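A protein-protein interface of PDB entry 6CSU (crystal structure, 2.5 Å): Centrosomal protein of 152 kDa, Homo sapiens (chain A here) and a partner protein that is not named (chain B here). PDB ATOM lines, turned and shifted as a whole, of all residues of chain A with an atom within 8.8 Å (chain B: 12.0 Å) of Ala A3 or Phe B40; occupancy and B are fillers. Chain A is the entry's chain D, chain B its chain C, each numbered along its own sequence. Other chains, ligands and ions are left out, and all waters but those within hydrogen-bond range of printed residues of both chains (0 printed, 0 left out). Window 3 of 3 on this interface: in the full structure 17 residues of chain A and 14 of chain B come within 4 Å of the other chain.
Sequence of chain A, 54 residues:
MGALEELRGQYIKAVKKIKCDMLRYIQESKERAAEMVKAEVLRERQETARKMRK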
ATOM      1  N   MET A   1     -37.699   3.081 -18.845  1.00  0.00           N
ATOM      2  CA  MET A   1     -38.053   1.876 -18.106  1.00  0.00           C
ATOM      3  C   MET A   1     -37.366   0.667 -18.730  1.00  0.00           C
ATOM      4  O   MET A   1     -36.632  -0.058 -18.060  1.00  0.00           O
ATOM      5  CB  MET A   1     -39.572   1.664 -18.085  1.00  0.00           C
ATOM      6  CG  MET A   1     -40.391   2.880 -18.500  1.00  0.00           C
ATOM      7  SD  MET A   1     -42.178   2.622 -18.473  1.00  0.00           S
ATOM      8  CE  MET A   1     -42.445   2.370 -16.725  1.00  0.00           C
ATOM      9  N   GLY A   2     -37.621   0.451 -20.023  1.00  0.00           N
ATOM     10  CA  GLY A   2     -36.964  -0.636 -20.729  1.00  0.00           C
ATOM     11  C   GLY A   2     -35.468  -0.435 -20.871  1.00  0.00           C
ATOM     12  O   GLY A   2     -34.702  -1.404 -20.838  1.00  0.00           O
ATOM     13  N   ALA A   3     -35.030   0.816 -21.038  1.00  0.00           N
ATOM     14  CA  ALA A   3     -33.601   1.102 -21.050  1.00  0.00           C
ATOM     15  C   ALA A   3     -32.959   0.717 -19.725  1.00  0.00           C
ATOM     16  O   ALA A   3     -31.845   0.185 -19.698  1.00  0.00           O
ATOM     17  CB  ALA A   3     -33.357   2.580 -21.352  1.00  0.00           C
ATOM     18  N   LEU A   4     -33.655   0.974 -18.615  1.00  0.00           N
ATOM     19  CA  LEU A   4     -33.131   0.621 -17.298  1.00  0.00           C
ATOM     20  C   LEU A   4     -32.954  -0.886 -17.163  1.00  0.00           C
ATOM     21  O   LEU A   4     -31.939  -1.361 -16.639  1.00  0.00           O
ATOM     22  CB  LEU A   4     -34.063   1.158 -16.207  1.00  0.00           C
ATOM     23  CG  LEU A   4     -33.879   2.574 -15.641  1.00  0.00           C
ATOM     24  CD1 LEU A   4     -33.496   3.583 -16.707  1.00  0.00           C
ATOM     25  CD2 LEU A   4     -35.150   3.017 -14.939  1.00  0.00           C
ATOM     26  N   GLU A   5     -33.936  -1.658 -17.636  1.00  0.00           N
ATOM     27  CA  GLU A   5     -33.835  -3.113 -17.582  1.00  0.00           C
ATOM     28  C   GLU A   5     -32.714  -3.613 -18.485  1.00  0.00           C
ATOM     29  O   GLU A   5     -31.953  -4.514 -18.110  1.00  0.00           O
ATOM     30  CB  GLU A   5     -35.176  -3.741 -17.972  1.00  0.00           C
ATOM     31  CG  GLU A   5     -35.283  -5.250 -17.790  1.00  0.00           C
ATOM     32  CD  GLU A   5     -34.616  -6.035 -18.905  1.00  0.00           C
ATOM     33  OE1 GLU A   5     -34.055  -7.112 -18.610  1.00  0.00           O
ATOM     34  OE2 GLU A   5     -34.645  -5.573 -20.066  1.00  0.00           O
ATOM     35  N   GLU A   6     -32.604  -3.046 -19.688  1.00  0.00           N
ATOM     36  CA  GLU A   6     -31.533  -3.427 -20.602  1.00  0.00           C
ATOM     37  C   GLU A   6     -30.169  -3.179 -19.976  1.00  0.00           C
ATOM     38  O   GLU A   6     -29.321  -4.075 -19.923  1.00  0.00           O
ATOM     39  CB  GLU A   6     -31.656  -2.655 -21.916  1.00  0.00           C
ATOM     40  CG  GLU A   6     -32.535  -3.308 -22.964  1.00  0.00           C
ATOM     41  CD  GLU A   6     -32.478  -2.576 -24.295  1.00  0.00           C
ATOM     42  OE1 GLU A   6     -33.503  -2.553 -25.010  1.00  0.00           O
ATOM     43  OE2 GLU A   6     -31.408  -2.017 -24.623  1.00  0.00           O
ATOM     44  N   LEU A   7     -29.940  -1.947 -19.510  1.00  0.00           N
ATOM     45  CA  LEU A   7     -28.650  -1.611 -18.921  1.00  0.00           C
ATOM     46  C   LEU A   7     -28.351  -2.496 -17.723  1.00  0.00           C
ATOM     47  O   LEU A   7     -27.217  -2.958 -17.551  1.00  0.00           O
ATOM     48  CB  LEU A   7     -28.624  -0.138 -18.516  1.00  0.00           C
ATOM     49  CG  LEU A   7     -28.607   0.898 -19.641  1.00  0.00           C
ATOM     50  CD1 LEU A   7     -28.519   2.311 -19.069  1.00  0.00           C
ATOM     51  CD2 LEU A   7     -27.460   0.627 -20.599  1.00  0.00           C
ATOM     52  N   ARG A   8     -29.359  -2.744 -16.886  1.00  0.00           N
ATOM     53  CA  ARG A   8     -29.194  -3.668 -15.773  1.00  0.00           C
ATOM     54  C   ARG A   8     -28.856  -5.062 -16.273  1.00  0.00           C
ATOM     55  O   ARG A   8     -28.014  -5.752 -15.689  1.00  0.00           O
ATOM     56  CB  ARG A   8     -30.471  -3.696 -14.936  1.00  0.00           C
ATOM     57  CG  ARG A   8     -30.366  -4.416 -13.612  1.00  0.00           C
ATOM     58  CD  ARG A   8     -31.753  -4.640 -13.033  1.00  0.00           C
ATOM     59  NE  ARG A   8     -32.176  -6.030 -13.177  1.00  0.00           N
ATOM     60  CZ  ARG A   8     -32.012  -6.956 -12.238  1.00  0.00           C
ATOM     61  NH1 ARG A   8     -31.438  -6.636 -11.084  1.00  0.00           N
ATOM     62  NH2 ARG A   8     -32.423  -8.198 -12.450  1.00  0.00           N
ATOM     63  N   GLY A   9     -29.499  -5.490 -17.359  1.00  0.00           N
ATOM     64  CA  GLY A   9     -29.224  -6.809 -17.893  1.00  0.00           C
ATOM     65  C   GLY A   9     -27.813  -6.926 -18.439  1.00  0.00           C
ATOM     66  O   GLY A   9     -27.169  -7.968 -18.306  1.00  0.00           O
ATOM     67  N   GLN A  10     -27.316  -5.847 -19.046  1.00  0.00           N
ATOM     68  CA  GLN A  10     -25.974  -5.870 -19.616  1.00  0.00           C
ATOM     69  C   GLN A  10     -24.913  -5.889 -18.527  1.00  0.00           C
ATOM     70  O   GLN A  10     -23.890  -6.570 -18.663  1.00  0.00           O
ATOM     71  CB  GLN A  10     -25.777  -4.666 -20.533  1.00  0.00           C
ATOM     72  CG  GLN A  10     -26.678  -4.647 -21.752  1.00  0.00           C
ATOM     73  CD  GLN A  10     -26.808  -3.262 -22.348  1.00  0.00           C
ATOM     74  OE1 GLN A  10     -26.327  -2.283 -21.778  1.00  0.00           O
ATOM     75  NE2 GLN A  10     -27.465  -3.170 -23.501  1.00  0.00           N
ATOM     76  N   LEU B  29     -19.696  -4.668 -22.928  1.00  0.00           N
ATOM     77  CA  LEU B  29     -20.635  -3.882 -22.136  1.00  0.00           C
ATOM     78  C   LEU B  29     -20.675  -2.441 -22.621  1.00  0.00           C
ATOM     79  O   LEU B  29     -21.751  -1.838 -22.713  1.00  0.00           O
ATOM     80  CB  LEU B  29     -20.256  -3.937 -20.657  1.00  0.00           C
ATOM     81  CG  LEU B  29     -21.068  -3.047 -19.710  1.00  0.00           C
ATOM     82  CD1 LEU B  29     -22.493  -3.559 -19.598  1.00  0.00           C
ATOM     83  CD2 LEU B  29     -20.413  -2.962 -18.332  1.00  0.00           C
ATOM     84  N   ARG B  31     -20.108  -1.333 -25.619  1.00  0.00           N
ATOM     85  CA  ARG B  31     -20.794  -1.244 -26.903  1.00  0.00           C
ATOM     86  C   ARG B  31     -22.292  -1.467 -26.753  1.00  0.00           C
ATOM     87  O   ARG B  31     -23.097  -0.737 -27.343  1.00  0.00           O
ATOM     88  CB  ARG B  31     -20.194  -2.248 -27.889  1.00  0.00           C
ATOM     89  CG  ARG B  31     -19.099  -1.658 -28.763  1.00  0.00           C
ATOM     90  CD  ARG B  31     -18.436  -2.694 -29.666  1.00  0.00           C
ATOM     91  NE  ARG B  31     -17.527  -3.574 -28.936  1.00  0.00           N
ATOM     92  CZ  ARG B  31     -17.772  -4.857 -28.695  1.00  0.00           C
ATOM     93  NH1 ARG B  31     -18.896  -5.406 -29.134  1.00  0.00           N
ATOM     94  NH2 ARG B  31     -16.895  -5.591 -28.023  1.00  0.00           N
ATOM     95  N   GLU B  32     -22.686  -2.475 -25.971  1.00  0.00           N
ATOM     96  CA  GLU B  32     -24.106  -2.743 -25.774  1.00  0.00           C
ATOM     97  C   GLU B  32     -24.800  -1.575 -25.086  1.00  0.00           C
ATOM     98  O   GLU B  32     -25.904  -1.183 -25.481  1.00  0.00           O
ATOM     99  CB  GLU B  32     -24.294  -4.021 -24.960  1.00  0.00           C
ATOM    100  CG  GLU B  32     -23.894  -5.294 -25.678  1.00  0.00           C
ATOM    101  CD  GLU B  32     -24.048  -6.523 -24.799  1.00  0.00           C
ATOM    102  OE1 GLU B  32     -23.826  -6.412 -23.575  1.00  0.00           O
ATOM    103  OE2 GLU B  32     -24.402  -7.593 -25.332  1.00  0.00           O
ATOM    104  N   SER B  33     -24.169  -1.008 -24.058  1.00  0.00           N
ATOM    105  CA  SER B  33     -24.802   0.068 -23.304  1.00  0.00           C
ATOM    106  C   SER B  33     -24.854   1.362 -24.107  1.00  0.00           C
ATOM    107  O   SER B  33     -25.863   2.076 -24.067  1.00  0.00           O
ATOM    108  CB  SER B  33     -24.066   0.287 -21.983  1.00  0.00           C
ATOM    109  OG  SER B  33     -22.754   0.762 -22.213  1.00  0.00           O
ATOM    110  N   GLU B  34     -23.777   1.676 -24.833  1.00  0.00           N
ATOM    111  CA  GLU B  34     -23.779   2.855 -25.693  1.00  0.00           C
ATOM    112  C   GLU B  34     -24.930   2.806 -26.689  1.00  0.00           C
ATOM    113  O   GLU B  34     -25.567   3.828 -26.972  1.00  0.00           O
ATOM    114  CB  GLU B  34     -22.437   2.967 -26.418  1.00  0.00           C
ATOM    115  CG  GLU B  34     -22.337   4.099 -27.429  1.00  0.00           C
ATOM    116  CD  GLU B  34     -20.918   4.291 -27.957  1.00  0.00           C
ATOM    117  OE1 GLU B  34     -20.531   3.596 -28.923  1.00  0.00           O
ATOM    118  OE2 GLU B  34     -20.186   5.133 -27.394  1.00  0.00           O
ATOM    119  N   LYS B  35     -25.228   1.617 -27.217  1.00  0.00           N
ATOM    120  CA  LYS B  35     -26.310   1.502 -28.186  1.00  0.00           C
ATOM    121  C   LYS B  35     -27.665   1.680 -27.519  1.00  0.00           C
ATOM    122  O   LYS B  35     -28.545   2.362 -28.060  1.00  0.00           O
ATOM    123  CB  LYS B  35     -26.246   0.156 -28.904  1.00  0.00           C
ATOM    124  CG  LYS B  35     -27.268   0.031 -30.025  1.00  0.00           C
ATOM    125  CD  LYS B  35     -27.796  -1.385 -30.160  1.00  0.00           C
ATOM    126  CE  LYS B  35     -26.972  -2.194 -31.144  1.00  0.00           C
ATOM    127  NZ  LYS B  35     -27.264  -3.652 -31.032  1.00  0.00           N
ATOM    128  N   THR B  36     -27.852   1.072 -26.344  1.00  0.00           N
ATOM    129  CA  THR B  36     -29.091   1.262 -25.597  1.00  0.00           C
ATOM    130  C   THR B  36     -29.340   2.738 -25.318  1.00  0.00           C
ATOM    131  O   THR B  36     -30.451   3.243 -25.517  1.00  0.00           O
ATOM    132  CB  THR B  36     -29.040   0.466 -24.291  1.00  0.00           C
ATOM    133  OG1 THR B  36     -29.104  -0.935 -24.579  1.00  0.00           O
ATOM    134  CG2 THR B  36     -30.203   0.839 -23.399  1.00  0.00           C
ATOM    135  N   VAL B  37     -28.305   3.453 -24.875  1.00  0.00           N
ATOM    136  CA  VAL B  37     -28.441   4.875 -24.574  1.00  0.00           C
ATOM    137  C   VAL B  37     -28.826   5.649 -25.831  1.00  0.00           C
ATOM    138  O   VAL B  37     -29.826   6.373 -25.852  1.00  0.00           O
ATOM    139  CB  VAL B  37     -27.143   5.423 -23.962  1.00  0.00           C
ATOM    140  CG1 VAL B  37     -27.229   6.930 -23.821  1.00  0.00           C
ATOM    141  CG2 VAL B  37     -26.875   4.767 -22.615  1.00  0.00           C
ATOM    142  N   ARG B  38     -28.028   5.499 -26.887  1.00  0.00           N
ATOM    143  CA  ARG B  38     -28.249   6.233 -28.131  1.00  0.00           C
ATOM    144  C   ARG B  38     -29.675   6.065 -28.636  1.00  0.00           C
ATOM    145  O   ARG B  38     -30.335   7.043 -29.011  1.00  0.00           O
ATOM    146  CB  ARG B  38     -27.256   5.750 -29.189  1.00  0.00           C
ATOM    147  CG  ARG B  38     -27.463   6.350 -30.566  1.00  0.00           C
ATOM    148  CD  ARG B  38     -26.791   5.520 -31.656  1.00  0.00           C
ATOM    149  NE  ARG B  38     -25.536   4.916 -31.212  1.00  0.00           N
ATOM    150  CZ  ARG B  38     -25.304   3.606 -31.165  1.00  0.00           C
ATOM    151  NH1 ARG B  38     -26.233   2.742 -31.549  1.00  0.00           N
ATOM    152  NH2 ARG B  38     -24.129   3.160 -30.747  1.00  0.00           N
ATOM    153  N   GLN B  39     -30.173   4.828 -28.633  1.00  0.00           N
ATOM    154  CA  GLN B  39     -31.450   4.535 -29.275  1.00  0.00           C
ATOM    155  C   GLN B  39     -32.627   4.963 -28.404  1.00  0.00           C
ATOM    156  O   GLN B  39     -33.601   5.537 -28.902  1.00  0.00           O
ATOM    157  CB  GLN B  39     -31.518   3.047 -29.624  1.00  0.00           C
ATOM    158  CG  GLN B  39     -30.498   2.638 -30.678  1.00  0.00           C
ATOM    159  CD  GLN B  39     -30.724   1.243 -31.224  1.00  0.00           C
ATOM    160  OE1 GLN B  39     -31.337   0.395 -30.571  1.00  0.00           O
ATOM    161  NE2 GLN B  39     -30.220   0.994 -32.430  1.00  0.00           N
ATOM    162  N   PHE B  40     -32.554   4.701 -27.095  1.00  0.00           N
ATOM    163  CA  PHE B  40     -33.595   5.182 -26.191  1.00  0.00           C
ATOM    164  C   PHE B  40     -33.579   6.702 -26.057  1.00  0.00           C
ATOM    165  O   PHE B  40     -34.632   7.305 -25.830  1.00  0.00           O
ATOM    166  CB  PHE B  40     -33.451   4.525 -24.814  1.00  0.00           C
ATOM    167  CG  PHE B  40     -34.047   3.138 -24.730  1.00  0.00           C
ATOM    168  CD1 PHE B  40     -35.411   2.972 -24.558  1.00  0.00           C
ATOM    169  CD2 PHE B  40     -33.242   2.005 -24.816  1.00  0.00           C
ATOM    170  CE1 PHE B  40     -35.969   1.708 -24.478  1.00  0.00           C
ATOM    171  CE2 PHE B  40     -33.795   0.734 -24.735  1.00  0.00           C
ATOM    172  CZ  PHE B  40     -35.163   0.589 -24.568  1.00  0.00           C
ATOM    173  N   THR B  41     -32.411   7.331 -26.199  1.00  0.00           N
ATOM    174  CA  THR B  41     -32.316   8.786 -26.205  1.00  0.00           C
ATOM    175  C   THR B  41     -32.990   9.395 -27.427  1.00  0.00           C
ATOM    176  O   THR B  41     -33.478  10.528 -27.353  1.00  0.00           O
ATOM    177  CB  THR B  41     -30.837   9.199 -26.115  1.00  0.00           C
ATOM    178  OG1 THR B  41     -30.433   9.205 -24.742  1.00  0.00           O
ATOM    179  CG2 THR B  41     -30.571  10.563 -26.728  1.00  0.00           C
ATOM    180  N   ALA B  42     -33.058   8.658 -28.537  1.00  0.00           N
ATOM    181  CA  ALA B  42     -33.816   9.131 -29.689  1.00  0.00           C
ATOM    182  C   ALA B  42     -35.290   9.302 -29.349  1.00  0.00           C
ATOM    183  O   ALA B  42     -35.949  10.194 -29.894  1.00  0.00           O
ATOM    184  CB  ALA B  42     -33.645   8.167 -30.865  1.00  0.00           C
ATOM    185  N   LEU B  43     -35.821   8.474 -28.451  1.00  0.00           N
ATOM    186  CA  LEU B  43     -37.206   8.611 -28.003  1.00  0.00           C
ATOM    187  C   LEU B  43     -37.440   9.983 -27.379  1.00  0.00           C
ATOM    188  O   LEU B  43     -38.427  10.649 -27.685  1.00  0.00           O
ATOM    189  CB  LEU B  43     -37.567   7.512 -27.000  1.00  0.00           C
ATOM    190  CG  LEU B  43     -37.623   6.075 -27.510  1.00  0.00           C
ATOM    191  CD1 LEU B  43     -37.955   5.113 -26.381  1.00  0.00           C
ATOM    192  CD2 LEU B  43     -38.653   5.961 -28.605  1.00  0.00           C
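The side-chain amide nitrogen (NE2) of Gln A10 sits at hydrogen-bond distance from the side-chain hydroxyl (OG1) of Thr B36, at 3.0 Å.
O of Glu B32 lies within hydrogen-bond range of NE2 of Gln A10 (3.2 Å).
The side-chain amide oxygen of Gln A10 lies close to the backbone NH of Ser B33, 3.4 Å away.
The side-chain carboxylate of Glu A6 lies within hydrogen-bond range of the side-chain hydroxyl of Thr B36.
The backbone carbonyl oxygen (O) of Leu B29 is in hydrogen-bond range of the side-chain hydroxyl (OG) of Ser B33 (2.8 Å).
O of Glu B32 lies within hydrogen-bond range of OG1 of Thr B36, at 3.3 Å.
Gly A2 touches Phe B40.
Phe B40 touches Ala A3.
CE2 of Phe B40 touches OE1 of Glu A6, 3.3 Å away.
CD2 of Leu A7 touches CB of Ser B33, 3.7 Å away.
Thr B36 touches Leu A7.
Leu B29 touches Gln A10.
Printed residues of chain B within 4 Å of Gly A2: Phe B40.
Ala A3 touches just one residue of chain B: Phe B40 (3.5 Å).
No residue of chain B comes within 4 Å of Leu A4.
No residue of chain B comes within 4 Å of Glu A5.
Of chain B, only Thr B36 (2.5 Å) and Phe B40 (3.3 Å) come within 4 Å of Glu A6.
Leu A7 touches just these residues of chain B: Ser B33 and Thr B36.
Gly A9 touches none of the printed residues of chain B.
Of the printed residues of chain A, Leu B29 touches Gln A10.
Of the printed residues of chain A, Thr B36 touches Glu A6 (2.5 Å), Leu A7 (3.9 Å) and Gln A10 (3.0 Å).
Arg B38 touches none of the printed residues of chain A.
Of the printed residues of chain A, Phe B40 touches Gly A2 (3.8 Å), Ala A3 (3.5 Å) and Glu A6 (3.3 Å).
The nearest printed residue of chain B that does not touch Gln A10 is Glu B34 (5.6 Å).
Hydrophobic or aromatic side chains of chain B that line the printed part of chain A: Leu B29 and Phe B40.
Among the printed residues, no Asp or Glu carboxylate lies within 4 Å of a Lys or Arg side-chain nitrogen of the other chain.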
